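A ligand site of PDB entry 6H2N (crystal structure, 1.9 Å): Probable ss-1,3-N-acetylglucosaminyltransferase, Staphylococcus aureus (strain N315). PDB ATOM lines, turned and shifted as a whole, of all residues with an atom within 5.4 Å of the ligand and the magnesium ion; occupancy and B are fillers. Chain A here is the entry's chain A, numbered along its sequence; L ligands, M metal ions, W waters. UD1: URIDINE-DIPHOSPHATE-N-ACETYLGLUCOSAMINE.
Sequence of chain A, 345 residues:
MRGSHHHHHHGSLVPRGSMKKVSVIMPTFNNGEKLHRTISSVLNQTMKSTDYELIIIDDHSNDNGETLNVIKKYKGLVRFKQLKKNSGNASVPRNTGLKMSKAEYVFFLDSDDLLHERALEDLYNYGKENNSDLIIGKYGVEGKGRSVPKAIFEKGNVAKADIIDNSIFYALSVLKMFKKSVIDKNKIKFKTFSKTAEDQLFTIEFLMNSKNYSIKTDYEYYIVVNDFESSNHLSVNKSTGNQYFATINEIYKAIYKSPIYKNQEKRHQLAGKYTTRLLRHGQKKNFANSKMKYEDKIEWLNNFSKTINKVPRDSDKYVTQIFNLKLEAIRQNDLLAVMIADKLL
The side-chain carboxylate (OD2) of Asp 199 lies within hydrogen-bond range of an oxygen (O6') of the ligand (2.6 Å). The backbone carbonyl oxygen (O) of Pro 27 is in hydrogen-bond range of an oxygen (O3B) of the ligand (2.7 Å). An oxygen (O4') of the ligand sits at hydrogen-bond distance from the side-chain carboxylate of Asp 110 (2.9 Å). The side-chain carboxylate (OD2) of Asp 59 lies within hydrogen-bond range of a nitrogen (N3) of the ligand (2.9 Å). An oxygen (O3B) of the ligand is in hydrogen-bond range of the backbone NH (N) of Ser 111. The side-chain hydroxyl (OG) of Ser 111 is in hydrogen-bond range of an oxygen (O2') of the ligand, at 2.9 Å. An oxygen (O4') of the ligand sits at hydrogen-bond distance from the guanidinium group (NH2) of Arg 94 (3.2 Å). N3 of the ligand is in hydrogen-bond range of O of Asn 89, 3.5 Å away. An oxygen (O4) of the ligand lies close to the side-chain amide oxygen (OD1) of Asn 86.
NH1 of Arg 94 is in salt-bridge range of OD1 of Asp 199 (2.9 Å). The guanidinium group (NH2) of Arg 94 lies within salt-bridge range of the side-chain carboxylate (OD1) of Asp 110 (2.8 Å). N of Asp 59 is in hydrogen-bond range of O of Thr 28 (2.8 Å). The side-chain hydroxyl of Ser 87 is in hydrogen-bond range of the side-chain carboxylate of Asp 59 (2.6 Å). The side-chain hydroxyl (OG) of Ser 111 sits at hydrogen-bond distance from the side-chain amide nitrogen (ND2) of Asn 31 (2.8 Å). The backbone NH of Gly 88 is in hydrogen-bond range of the side-chain amide oxygen of Asn 86 (3.3 Å). OD1 of Asp 113 lies within hydrogen-bond range of N of Val 225. OG of Ser 173 sits close to N of Leu 175 (3.3 Å).
An oxygen (O4) of the ligand lies close to the backbone carbonyl oxygen of Gly 88. Residues that only touch the ligand: Ala 90, Thr 28, Phe 29, Pro 93, Ser 173 and Leu 175. Hydrophobic or aromatic side chains that line the ligand: Pro 27, Phe 29, Ala 90, Pro 93 and Leu 175. The nearest printed residue that does not touch the ligand is Asn 31 (4.4 Å).
Residues that only touch the magnesium ion: Asp 113 and Val 225. Within 4 Å of the magnesium ion: Asp 112, Asp 113 and Val 225.
Water W1 is bound to the magnesium ion (2.1 Å). The magnesium ion is bound by O2A of the ligand. OD2 of Asp 112 is bound to the magnesium ion (2.3 Å). An oxygen (O1B) of the ligand binds the magnesium ion. OD1 of Asp 112 binds the magnesium ion, 2.4 Å away.
Water W1 bridges OD2 of Asp 110 and OD2 of Asp 113. Water W2 lies within hydrogen-bond range of the side-chain carboxylate of Asp 199, an oxygen (O4') of the ligand and the backbone NH of Val 174. Water W3 lies within hydrogen-bond range of O6' of the ligand and N of Ala 90.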
ATOM      1  N   MET A  26      -7.356  30.927 -27.142  1.00  0.00           N
ATOM      2  CA  MET A  26      -6.713  30.024 -26.170  1.00  0.00           C
ATOM      3  C   MET A  26      -6.550  30.716 -24.818  1.00  0.00           C
ATOM      4  O   MET A  26      -5.684  31.563 -24.651  1.00  0.00           O
ATOM      5  CB  MET A  26      -5.337  29.552 -26.646  1.00  0.00           C
ATOM      6  CG  MET A  26      -4.663  28.623 -25.653  1.00  0.00           C
ATOM      7  SD  MET A  26      -3.027  28.086 -26.168  1.00  0.00           S
ATOM      8  CE  MET A  26      -2.146  29.643 -26.048  1.00  0.00           C
ATOM      9  N   PRO A  27      -7.373  30.345 -23.801  1.00  0.00           N
ATOM     10  CA  PRO A  27      -7.136  30.768 -22.423  1.00  0.00           C
ATOM     11  C   PRO A  27      -5.942  30.042 -21.789  1.00  0.00           C
ATOM     12  O   PRO A  27      -5.774  28.849 -22.023  1.00  0.00           O
ATOM     13  CB  PRO A  27      -8.439  30.415 -21.684  1.00  0.00           C
ATOM     14  CG  PRO A  27      -9.427  30.074 -22.777  1.00  0.00           C
ATOM     15  CD  PRO A  27      -8.594  29.547 -23.924  1.00  0.00           C
ATOM     16  N   THR A  28      -5.137  30.767 -20.992  1.00  0.00           N
ATOM     17  CA  THR A  28      -3.976  30.194 -20.312  1.00  0.00           C
ATOM     18  C   THR A  28      -4.060  30.481 -18.810  1.00  0.00           C
ATOM     19  O   THR A  28      -4.672  31.472 -18.387  1.00  0.00           O
ATOM     20  CB  THR A  28      -2.654  30.734 -20.883  1.00  0.00           C
ATOM     21  OG1 THR A  28      -2.580  32.145 -20.675  1.00  0.00           O
ATOM     22  CG2 THR A  28      -2.482  30.425 -22.354  1.00  0.00           C
ATOM     23  N   PHE A  29      -3.437  29.608 -18.017  1.00  0.00           N
ATOM     24  CA  PHE A  29      -3.363  29.752 -16.570  1.00  0.00           C
ATOM     25  C   PHE A  29      -2.312  28.800 -15.984  1.00  0.00           C
ATOM     26  O   PHE A  29      -2.553  27.599 -15.857  1.00  0.00           O
ATOM     27  CB  PHE A  29      -4.727  29.496 -15.923  1.00  0.00           C
ATOM     28  CG  PHE A  29      -4.816  30.003 -14.504  1.00  0.00           C
ATOM     29  CD1 PHE A  29      -4.867  31.363 -14.251  1.00  0.00           C
ATOM     30  CD2 PHE A  29      -4.817  29.125 -13.425  1.00  0.00           C
ATOM     31  CE1 PHE A  29      -4.933  31.833 -12.945  1.00  0.00           C
ATOM     32  N   ASN A  31       0.641  27.535 -16.988  1.00  0.00           N
ATOM     33  CA  ASN A  31       0.949  26.414 -17.886  1.00  0.00           C
ATOM     34  C   ASN A  31       2.449  26.092 -17.851  1.00  0.00           C
ATOM     35  O   ASN A  31       2.830  24.920 -17.810  1.00  0.00           O
ATOM     36  CB  ASN A  31       0.498  26.706 -19.314  1.00  0.00           C
ATOM     37  CG  ASN A  31      -1.004  26.843 -19.428  1.00  0.00           C
ATOM     38  OD1 ASN A  31      -1.510  27.922 -19.729  1.00  0.00           O
ATOM     39  ND2 ASN A  31      -1.725  25.766 -19.181  1.00  0.00           N
ATOM     40  N   ASP A  59      -5.497  34.111 -17.791  1.00  0.00           N
ATOM     41  CA  ASP A  59      -6.458  34.343 -16.725  1.00  0.00           C
ATOM     42  C   ASP A  59      -5.729  34.792 -15.452  1.00  0.00           C
ATOM     43  O   ASP A  59      -5.935  34.213 -14.391  1.00  0.00           O
ATOM     44  CB  ASP A  59      -7.318  33.103 -16.471  1.00  0.00           C
ATOM     45  CG  ASP A  59      -8.648  33.434 -15.825  1.00  0.00           C
ATOM     46  OD1 ASP A  59      -8.881  34.637 -15.548  1.00  0.00           O
ATOM     47  OD2 ASP A  59      -9.448  32.494 -15.608  1.00  0.00           O
ATOM     48  N   ASN A  86      -7.932  36.567 -11.657  1.00  0.00           N
ATOM     49  CA  ASN A  86      -8.288  35.213 -12.041  1.00  0.00           C
ATOM     50  C   ASN A  86      -9.811  35.012 -11.973  1.00  0.00           C
ATOM     51  O   ASN A  86     -10.418  35.198 -10.930  1.00  0.00           O
ATOM     52  CB  ASN A  86      -7.587  34.186 -11.149  1.00  0.00           C
ATOM     53  CG  ASN A  86      -7.857  32.770 -11.598  1.00  0.00           C
ATOM     54  OD1 ASN A  86      -8.004  32.523 -12.792  1.00  0.00           O
ATOM     55  ND2 ASN A  86      -7.941  31.836 -10.658  1.00  0.00           N
ATOM     56  N   SER A  87     -10.411  34.623 -13.107  1.00  0.00           N
ATOM     57  CA  SER A  87     -11.846  34.349 -13.214  1.00  0.00           C
ATOM     58  C   SER A  87     -12.169  32.985 -12.607  1.00  0.00           C
ATOM     59  O   SER A  87     -13.272  32.804 -12.082  1.00  0.00           O
ATOM     60  CB  SER A  87     -12.327  34.427 -14.651  1.00  0.00           C
ATOM     61  OG  SER A  87     -11.882  33.313 -15.404  1.00  0.00           O
ATOM     62  N   GLY A  88     -11.241  32.031 -12.715  1.00  0.00           N
ATOM     63  CA  GLY A  88     -11.378  30.719 -12.072  1.00  0.00           C
ATOM     64  C   GLY A  88     -11.602  29.575 -13.058  1.00  0.00           C
ATOM     65  O   GLY A  88     -11.439  28.402 -12.701  1.00  0.00           O
ATOM     66  N   ASN A  89     -11.954  29.915 -14.311  1.00  0.00           N
ATOM     67  CA  ASN A  89     -12.137  28.928 -15.364  1.00  0.00           C
ATOM     68  C   ASN A  89     -12.118  29.661 -16.714  1.00  0.00           C
ATOM     69  O   ASN A  89     -11.883  30.856 -16.777  1.00  0.00           O
ATOM     70  CB  ASN A  89     -13.405  28.095 -15.137  1.00  0.00           C
ATOM     71  CG  ASN A  89     -14.674  28.923 -15.226  1.00  0.00           C
ATOM     72  OD1 ASN A  89     -14.819  29.751 -16.103  1.00  0.00           O
ATOM     73  ND2 ASN A  89     -15.601  28.697 -14.321  1.00  0.00           N
ATOM     74  N   ALA A  90     -12.378  28.914 -17.800  1.00  0.00           N
ATOM     75  CA  ALA A  90     -12.081  29.387 -19.136  1.00  0.00           C
ATOM     76  C   ALA A  90     -13.179  30.343 -19.655  1.00  0.00           C
ATOM     77  O   ALA A  90     -12.977  30.968 -20.672  1.00  0.00           O
ATOM     78  CB  ALA A  90     -11.885  28.211 -20.060  1.00  0.00           C
ATOM     79  N   PRO A  93     -12.353  34.505 -19.893  1.00  0.00           N
ATOM     80  CA  PRO A  93     -11.343  34.604 -20.941  1.00  0.00           C
ATOM     81  C   PRO A  93     -11.952  34.355 -22.333  1.00  0.00           C
ATOM     82  O   PRO A  93     -11.773  35.144 -23.207  1.00  0.00           O
ATOM     83  CB  PRO A  93     -10.308  33.538 -20.568  1.00  0.00           C
ATOM     84  CG  PRO A  93     -10.470  33.361 -19.069  1.00  0.00           C
ATOM     85  CD  PRO A  93     -11.931  33.646 -18.771  1.00  0.00           C
ATOM     86  N   ARG A  94     -12.709  33.261 -22.495  1.00  0.00           N
ATOM     87  CA  ARG A  94     -13.258  32.939 -23.797  1.00  0.00           C
ATOM     88  C   ARG A  94     -14.196  34.059 -24.270  1.00  0.00           C
ATOM     89  O   ARG A  94     -14.194  34.387 -25.459  1.00  0.00           O
ATOM     90  CB  ARG A  94     -13.986  31.596 -23.769  1.00  0.00           C
ATOM     91  CG  ARG A  94     -13.051  30.386 -23.727  1.00  0.00           C
ATOM     92  CD  ARG A  94     -13.833  29.107 -23.607  1.00  0.00           C
ATOM     93  NE  ARG A  94     -12.967  27.946 -23.508  1.00  0.00           N
ATOM     94  CZ  ARG A  94     -13.346  26.752 -23.074  1.00  0.00           C
ATOM     95  NH1 ARG A  94     -14.567  26.595 -22.598  1.00  0.00           N
ATOM     96  NH2 ARG A  94     -12.507  25.729 -23.135  1.00  0.00           N
ATOM     97  N   LEU A 109      -9.329  26.645 -28.227  1.00  0.00           N
ATOM     98  CA  LEU A 109      -8.224  25.724 -27.954  1.00  0.00           C
ATOM     99  C   LEU A 109      -7.771  25.856 -26.483  1.00  0.00           C
ATOM    100  O   LEU A 109      -7.378  26.932 -26.058  1.00  0.00           O
ATOM    101  CB  LEU A 109      -7.094  26.047 -28.935  1.00  0.00           C
ATOM    102  CG  LEU A 109      -5.730  25.437 -28.618  1.00  0.00           C
ATOM    103  CD1 LEU A 109      -5.792  23.927 -28.676  1.00  0.00           C
ATOM    104  CD2 LEU A 109      -4.661  25.974 -29.561  1.00  0.00           C
ATOM    105  N   ASP A 110      -7.872  24.764 -25.706  1.00  0.00           N
ATOM    106  CA  ASP A 110      -7.360  24.701 -24.320  1.00  0.00           C
ATOM    107  C   ASP A 110      -5.831  24.673 -24.372  1.00  0.00           C
ATOM    108  O   ASP A 110      -5.289  24.161 -25.325  1.00  0.00           O
ATOM    109  CB  ASP A 110      -7.888  23.486 -23.570  1.00  0.00           C
ATOM    110  CG  ASP A 110      -9.375  23.537 -23.305  1.00  0.00           C
ATOM    111  OD1 ASP A 110      -9.966  24.634 -23.528  1.00  0.00           O
ATOM    112  OD2 ASP A 110      -9.945  22.478 -22.888  1.00  0.00           O
ATOM    113  N   SER A 111      -5.182  25.186 -23.310  1.00  0.00           N
ATOM    114  CA  SER A 111      -3.777  25.595 -23.312  1.00  0.00           C
ATOM    115  C   SER A 111      -2.788  24.422 -23.161  1.00  0.00           C
ATOM    116  O   SER A 111      -1.573  24.656 -23.173  1.00  0.00           O
ATOM    117  CB  SER A 111      -3.519  26.610 -22.221  1.00  0.00           C
ATOM    118  OG  SER A 111      -3.825  26.055 -20.952  1.00  0.00           O
ATOM    119  N   ASP A 112      -3.278  23.197 -22.945  1.00  0.00           N
ATOM    120  CA  ASP A 112      -2.412  22.011 -22.844  1.00  0.00           C
ATOM    121  C   ASP A 112      -2.570  21.101 -24.090  1.00  0.00           C
ATOM    122  O   ASP A 112      -1.767  20.199 -24.286  1.00  0.00           O
ATOM    123  CB  ASP A 112      -2.665  21.237 -21.550  1.00  0.00           C
ATOM    124  CG  ASP A 112      -4.115  20.834 -21.305  1.00  0.00           C
ATOM    125  OD1 ASP A 112      -5.000  21.381 -22.016  1.00  0.00           O
ATOM    126  OD2 ASP A 112      -4.362  19.995 -20.401  1.00  0.00           O
ATOM    127  N   ASP A 113      -3.573  21.392 -24.930  1.00  0.00           N
ATOM    128  CA  ASP A 113      -3.949  20.547 -26.087  1.00  0.00           C
ATOM    129  C   ASP A 113      -3.094  20.937 -27.299  1.00  0.00           C
ATOM    130  O   ASP A 113      -2.296  21.887 -27.238  1.00  0.00           O
ATOM    131  CB  ASP A 113      -5.457  20.652 -26.345  1.00  0.00           C
ATOM    132  CG  ASP A 113      -6.299  20.136 -25.191  1.00  0.00           C
ATOM    133  OD1 ASP A 113      -5.787  19.254 -24.452  1.00  0.00           O
ATOM    134  OD2 ASP A 113      -7.451  20.627 -25.020  1.00  0.00           O
ATOM    135  N   SER A 173     -18.275  19.611 -25.994  1.00  0.00           N
ATOM    136  CA  SER A 173     -17.179  20.548 -25.703  1.00  0.00           C
ATOM    137  C   SER A 173     -17.134  21.618 -26.798  1.00  0.00           C
ATOM    138  O   SER A 173     -17.567  21.379 -27.938  1.00  0.00           O
ATOM    139  CB  SER A 173     -15.831  19.851 -25.579  1.00  0.00           C
ATOM    140  OG  SER A 173     -15.180  19.780 -26.841  1.00  0.00           O
ATOM    141  N   VAL A 174     -16.555  22.774 -26.484  1.00  0.00           N
ATOM    142  CA  VAL A 174     -16.479  23.907 -27.446  1.00  0.00           C
ATOM    143  C   VAL A 174     -15.172  23.847 -28.248  1.00  0.00           C
ATOM    144  O   VAL A 174     -14.779  24.849 -28.890  1.00  0.00           O
ATOM    145  CB  VAL A 174     -16.662  25.257 -26.734  1.00  0.00           C
ATOM    146  CG1 VAL A 174     -18.008  25.363 -26.046  1.00  0.00           C
ATOM    147  CG2 VAL A 174     -15.540  25.541 -25.741  1.00  0.00           C
ATOM    148  N   LEU A 175     -14.511  22.680 -28.245  1.00  0.00           N
ATOM    149  CA  LEU A 175     -13.231  22.503 -28.913  1.00  0.00           C
ATOM    150  C   LEU A 175     -13.506  22.155 -30.398  1.00  0.00           C
ATOM    151  O   LEU A 175     -13.207  21.064 -30.922  1.00  0.00           O
ATOM    152  CB  LEU A 175     -12.443  21.432 -28.155  1.00  0.00           C
ATOM    153  CG  LEU A 175     -12.286  21.693 -26.652  1.00  0.00           C
ATOM    154  CD1 LEU A 175     -11.518  20.588 -25.976  1.00  0.00           C
ATOM    155  CD2 LEU A 175     -11.627  23.043 -26.399  1.00  0.00           C
ATOM    156  N   GLU A 198     -20.932  24.623 -18.239  1.00  0.00           N
ATOM    157  CA  GLU A 198     -21.062  25.901 -18.914  1.00  0.00           C
ATOM    158  C   GLU A 198     -20.703  25.737 -20.404  1.00  0.00           C
ATOM    159  O   GLU A 198     -21.235  26.437 -21.266  1.00  0.00           O
ATOM    160  CB  GLU A 198     -20.218  26.947 -18.175  1.00  0.00           C
ATOM    161  CG  GLU A 198     -18.701  26.801 -18.366  1.00  0.00           C
ATOM    162  CD  GLU A 198     -17.924  26.197 -17.210  1.00  0.00           C
ATOM    163  N   ASP A 199     -19.788  24.803 -20.699  1.00  0.00           N
ATOM    164  CA  ASP A 199     -19.360  24.564 -22.076  1.00  0.00           C
ATOM    165  C   ASP A 199     -20.543  23.933 -22.838  1.00  0.00           C
ATOM    166  O   ASP A 199     -20.940  24.391 -23.915  1.00  0.00           O
ATOM    167  CB  ASP A 199     -18.047  23.771 -22.076  1.00  0.00           C
ATOM    168  CG  ASP A 199     -16.834  24.597 -21.636  1.00  0.00           C
ATOM    169  OD1 ASP A 199     -17.020  25.787 -21.325  1.00  0.00           O
ATOM    170  OD2 ASP A 199     -15.702  24.044 -21.589  1.00  0.00           O
ATOM    171  N   VAL A 224      -6.258  16.014 -27.319  1.00  0.00           N
ATOM    172  CA  VAL A 224      -6.484  16.266 -25.909  1.00  0.00           C
ATOM    173  C   VAL A 224      -5.341  15.619 -25.122  1.00  0.00           C
ATOM    174  O   VAL A 224      -5.173  14.380 -25.140  1.00  0.00           O
ATOM    175  CB  VAL A 224      -7.847  15.718 -25.455  1.00  0.00           C
ATOM    176  CG1 VAL A 224      -7.994  15.792 -23.943  1.00  0.00           C
ATOM    177  CG2 VAL A 224      -8.991  16.450 -26.139  1.00  0.00           C
ATOM    178  N   VAL A 225      -4.580  16.454 -24.405  1.00  0.00           N
ATOM    179  CA  VAL A 225      -3.490  16.017 -23.543  1.00  0.00           C
ATOM    180  C   VAL A 225      -4.006  15.897 -22.100  1.00  0.00           C
ATOM    181  O   VAL A 225      -4.643  16.824 -21.563  1.00  0.00           O
ATOM    182  CB  VAL A 225      -2.266  16.937 -23.659  1.00  0.00           C
ATOM    183  CG1 VAL A 225      -1.099  16.448 -22.817  1.00  0.00           C
ATOM    184  CG2 VAL A 225      -1.831  17.118 -25.109  1.00  0.00           C
ATOM    185  N   ASN A 226      -3.778  14.704 -21.519  1.00  0.00           N
ATOM    186  CA  ASN A 226      -4.040  14.340 -20.114  1.00  0.00           C
ATOM    187  C   ASN A 226      -2.702  14.116 -19.394  1.00  0.00           C
ATOM    188  O   ASN A 226      -2.459  14.611 -18.285  1.00  0.00           O
ATOM    189  CB  ASN A 226      -4.891  13.074 -20.023  1.00  0.00           C
ATOM    190  CG  ASN A 226      -6.200  13.162 -20.786  1.00  0.00           C
ATOM    191  OD1 ASN A 226      -6.878  14.196 -20.765  1.00  0.00           O
ATOM    192  ND2 ASN A 226      -6.583  12.077 -21.444  1.00  0.00           N
HETATM  193  C1' UD1 L   1     -11.934  20.428 -19.163  1.00  0.00           C
HETATM  194  C2' UD1 L   1     -12.616  19.641 -20.267  1.00  0.00           C
HETATM  195  C3' UD1 L   1     -12.564  20.406 -21.584  1.00  0.00           C
HETATM  196  C4' UD1 L   1     -13.059  21.842 -21.403  1.00  0.00           C
HETATM  197  C5' UD1 L   1     -12.402  22.514 -20.202  1.00  0.00           C
HETATM  198  C6' UD1 L   1     -12.999  23.883 -19.924  1.00  0.00           C
HETATM  199  C7' UD1 L   1     -12.687  17.182 -20.183  1.00  0.00           C
HETATM  200  C8' UD1 L   1     -11.927  15.911 -20.411  1.00  0.00           C
HETATM  201  N2' UD1 L   1     -12.017  18.318 -20.419  1.00  0.00           N
HETATM  202  O1' UD1 L   1     -10.556  20.587 -19.507  1.00  0.00           O
HETATM  203  O3' UD1 L   1     -13.363  19.720 -22.548  1.00  0.00           O
HETATM  204  O4' UD1 L   1     -12.780  22.617 -22.584  1.00  0.00           O
HETATM  205  O5' UD1 L   1     -12.529  21.708 -19.033  1.00  0.00           O
HETATM  206  O6' UD1 L   1     -14.306  23.715 -19.376  1.00  0.00           O
HETATM  207  O7' UD1 L   1     -13.856  17.172 -19.817  1.00  0.00           O
HETATM  208  N1  UD1 L   1      -8.291  27.928 -17.337  1.00  0.00           N
HETATM  209  C2  UD1 L   1      -8.684  29.264 -17.058  1.00  0.00           C
HETATM  210  N3  UD1 L   1      -8.768  29.713 -15.795  1.00  0.00           N
HETATM  211  C4  UD1 L   1      -8.463  28.897 -14.769  1.00  0.00           C
HETATM  212  C5  UD1 L   1      -8.076  27.577 -15.009  1.00  0.00           C
HETATM  213  C6  UD1 L   1      -8.001  27.103 -16.315  1.00  0.00           C
HETATM  214  O2  UD1 L   1      -8.975  30.050 -17.986  1.00  0.00           O
HETATM  215  O4  UD1 L   1      -8.537  29.332 -13.594  1.00  0.00           O
HETATM  216  C1B UD1 L   1      -8.233  27.476 -18.735  1.00  0.00           C
HETATM  217  C2B UD1 L   1      -7.009  26.633 -19.077  1.00  0.00           C
HETATM  218  O2' UD1 L   1      -5.861  27.440 -19.334  1.00  0.00           O
HETATM  219  C3B UD1 L   1      -7.510  25.892 -20.305  1.00  0.00           C
HETATM  220  C4B UD1 L   1      -8.988  25.674 -20.024  1.00  0.00           C
HETATM  221  O4B UD1 L   1      -9.352  26.656 -19.044  1.00  0.00           O
HETATM  222  O3B UD1 L   1      -7.389  26.705 -21.488  1.00  0.00           O
HETATM  223  C5B UD1 L   1      -9.275  24.279 -19.512  1.00  0.00           C
HETATM  224  O5B UD1 L   1      -8.232  23.884 -18.641  1.00  0.00           O
HETATM  225  PA  UD1 L   1      -7.618  22.409 -18.718  1.00  0.00           P
HETATM  226  O1A UD1 L   1      -6.456  22.290 -17.764  1.00  0.00           O
HETATM  227  O2A UD1 L   1      -7.427  22.000 -20.168  1.00  0.00           O
HETATM  228  O3A UD1 L   1      -8.884  21.641 -18.057  1.00  0.00           O
HETATM  229  PB  UD1 L   1      -9.385  20.179 -18.490  1.00  0.00           P
HETATM  230  O1B UD1 L   1      -8.276  19.486 -19.264  1.00  0.00           O
HETATM  231  O2B UD1 L   1     -10.009  19.495 -17.291  1.00  0.00           O
HETATM  232 MG    MG M   1      -6.647  20.078 -20.863  1.00  0.00          MG
HETATM  233  O   HOH W   1      -8.259  20.535 -22.197  1.00  0.00           O
HETATM  234  O   HOH W   2     -15.358  22.636 -23.741  1.00  0.00           O
HETATM  235  O   HOH W   3     -13.649  26.018 -17.645  1.00  0.00           O
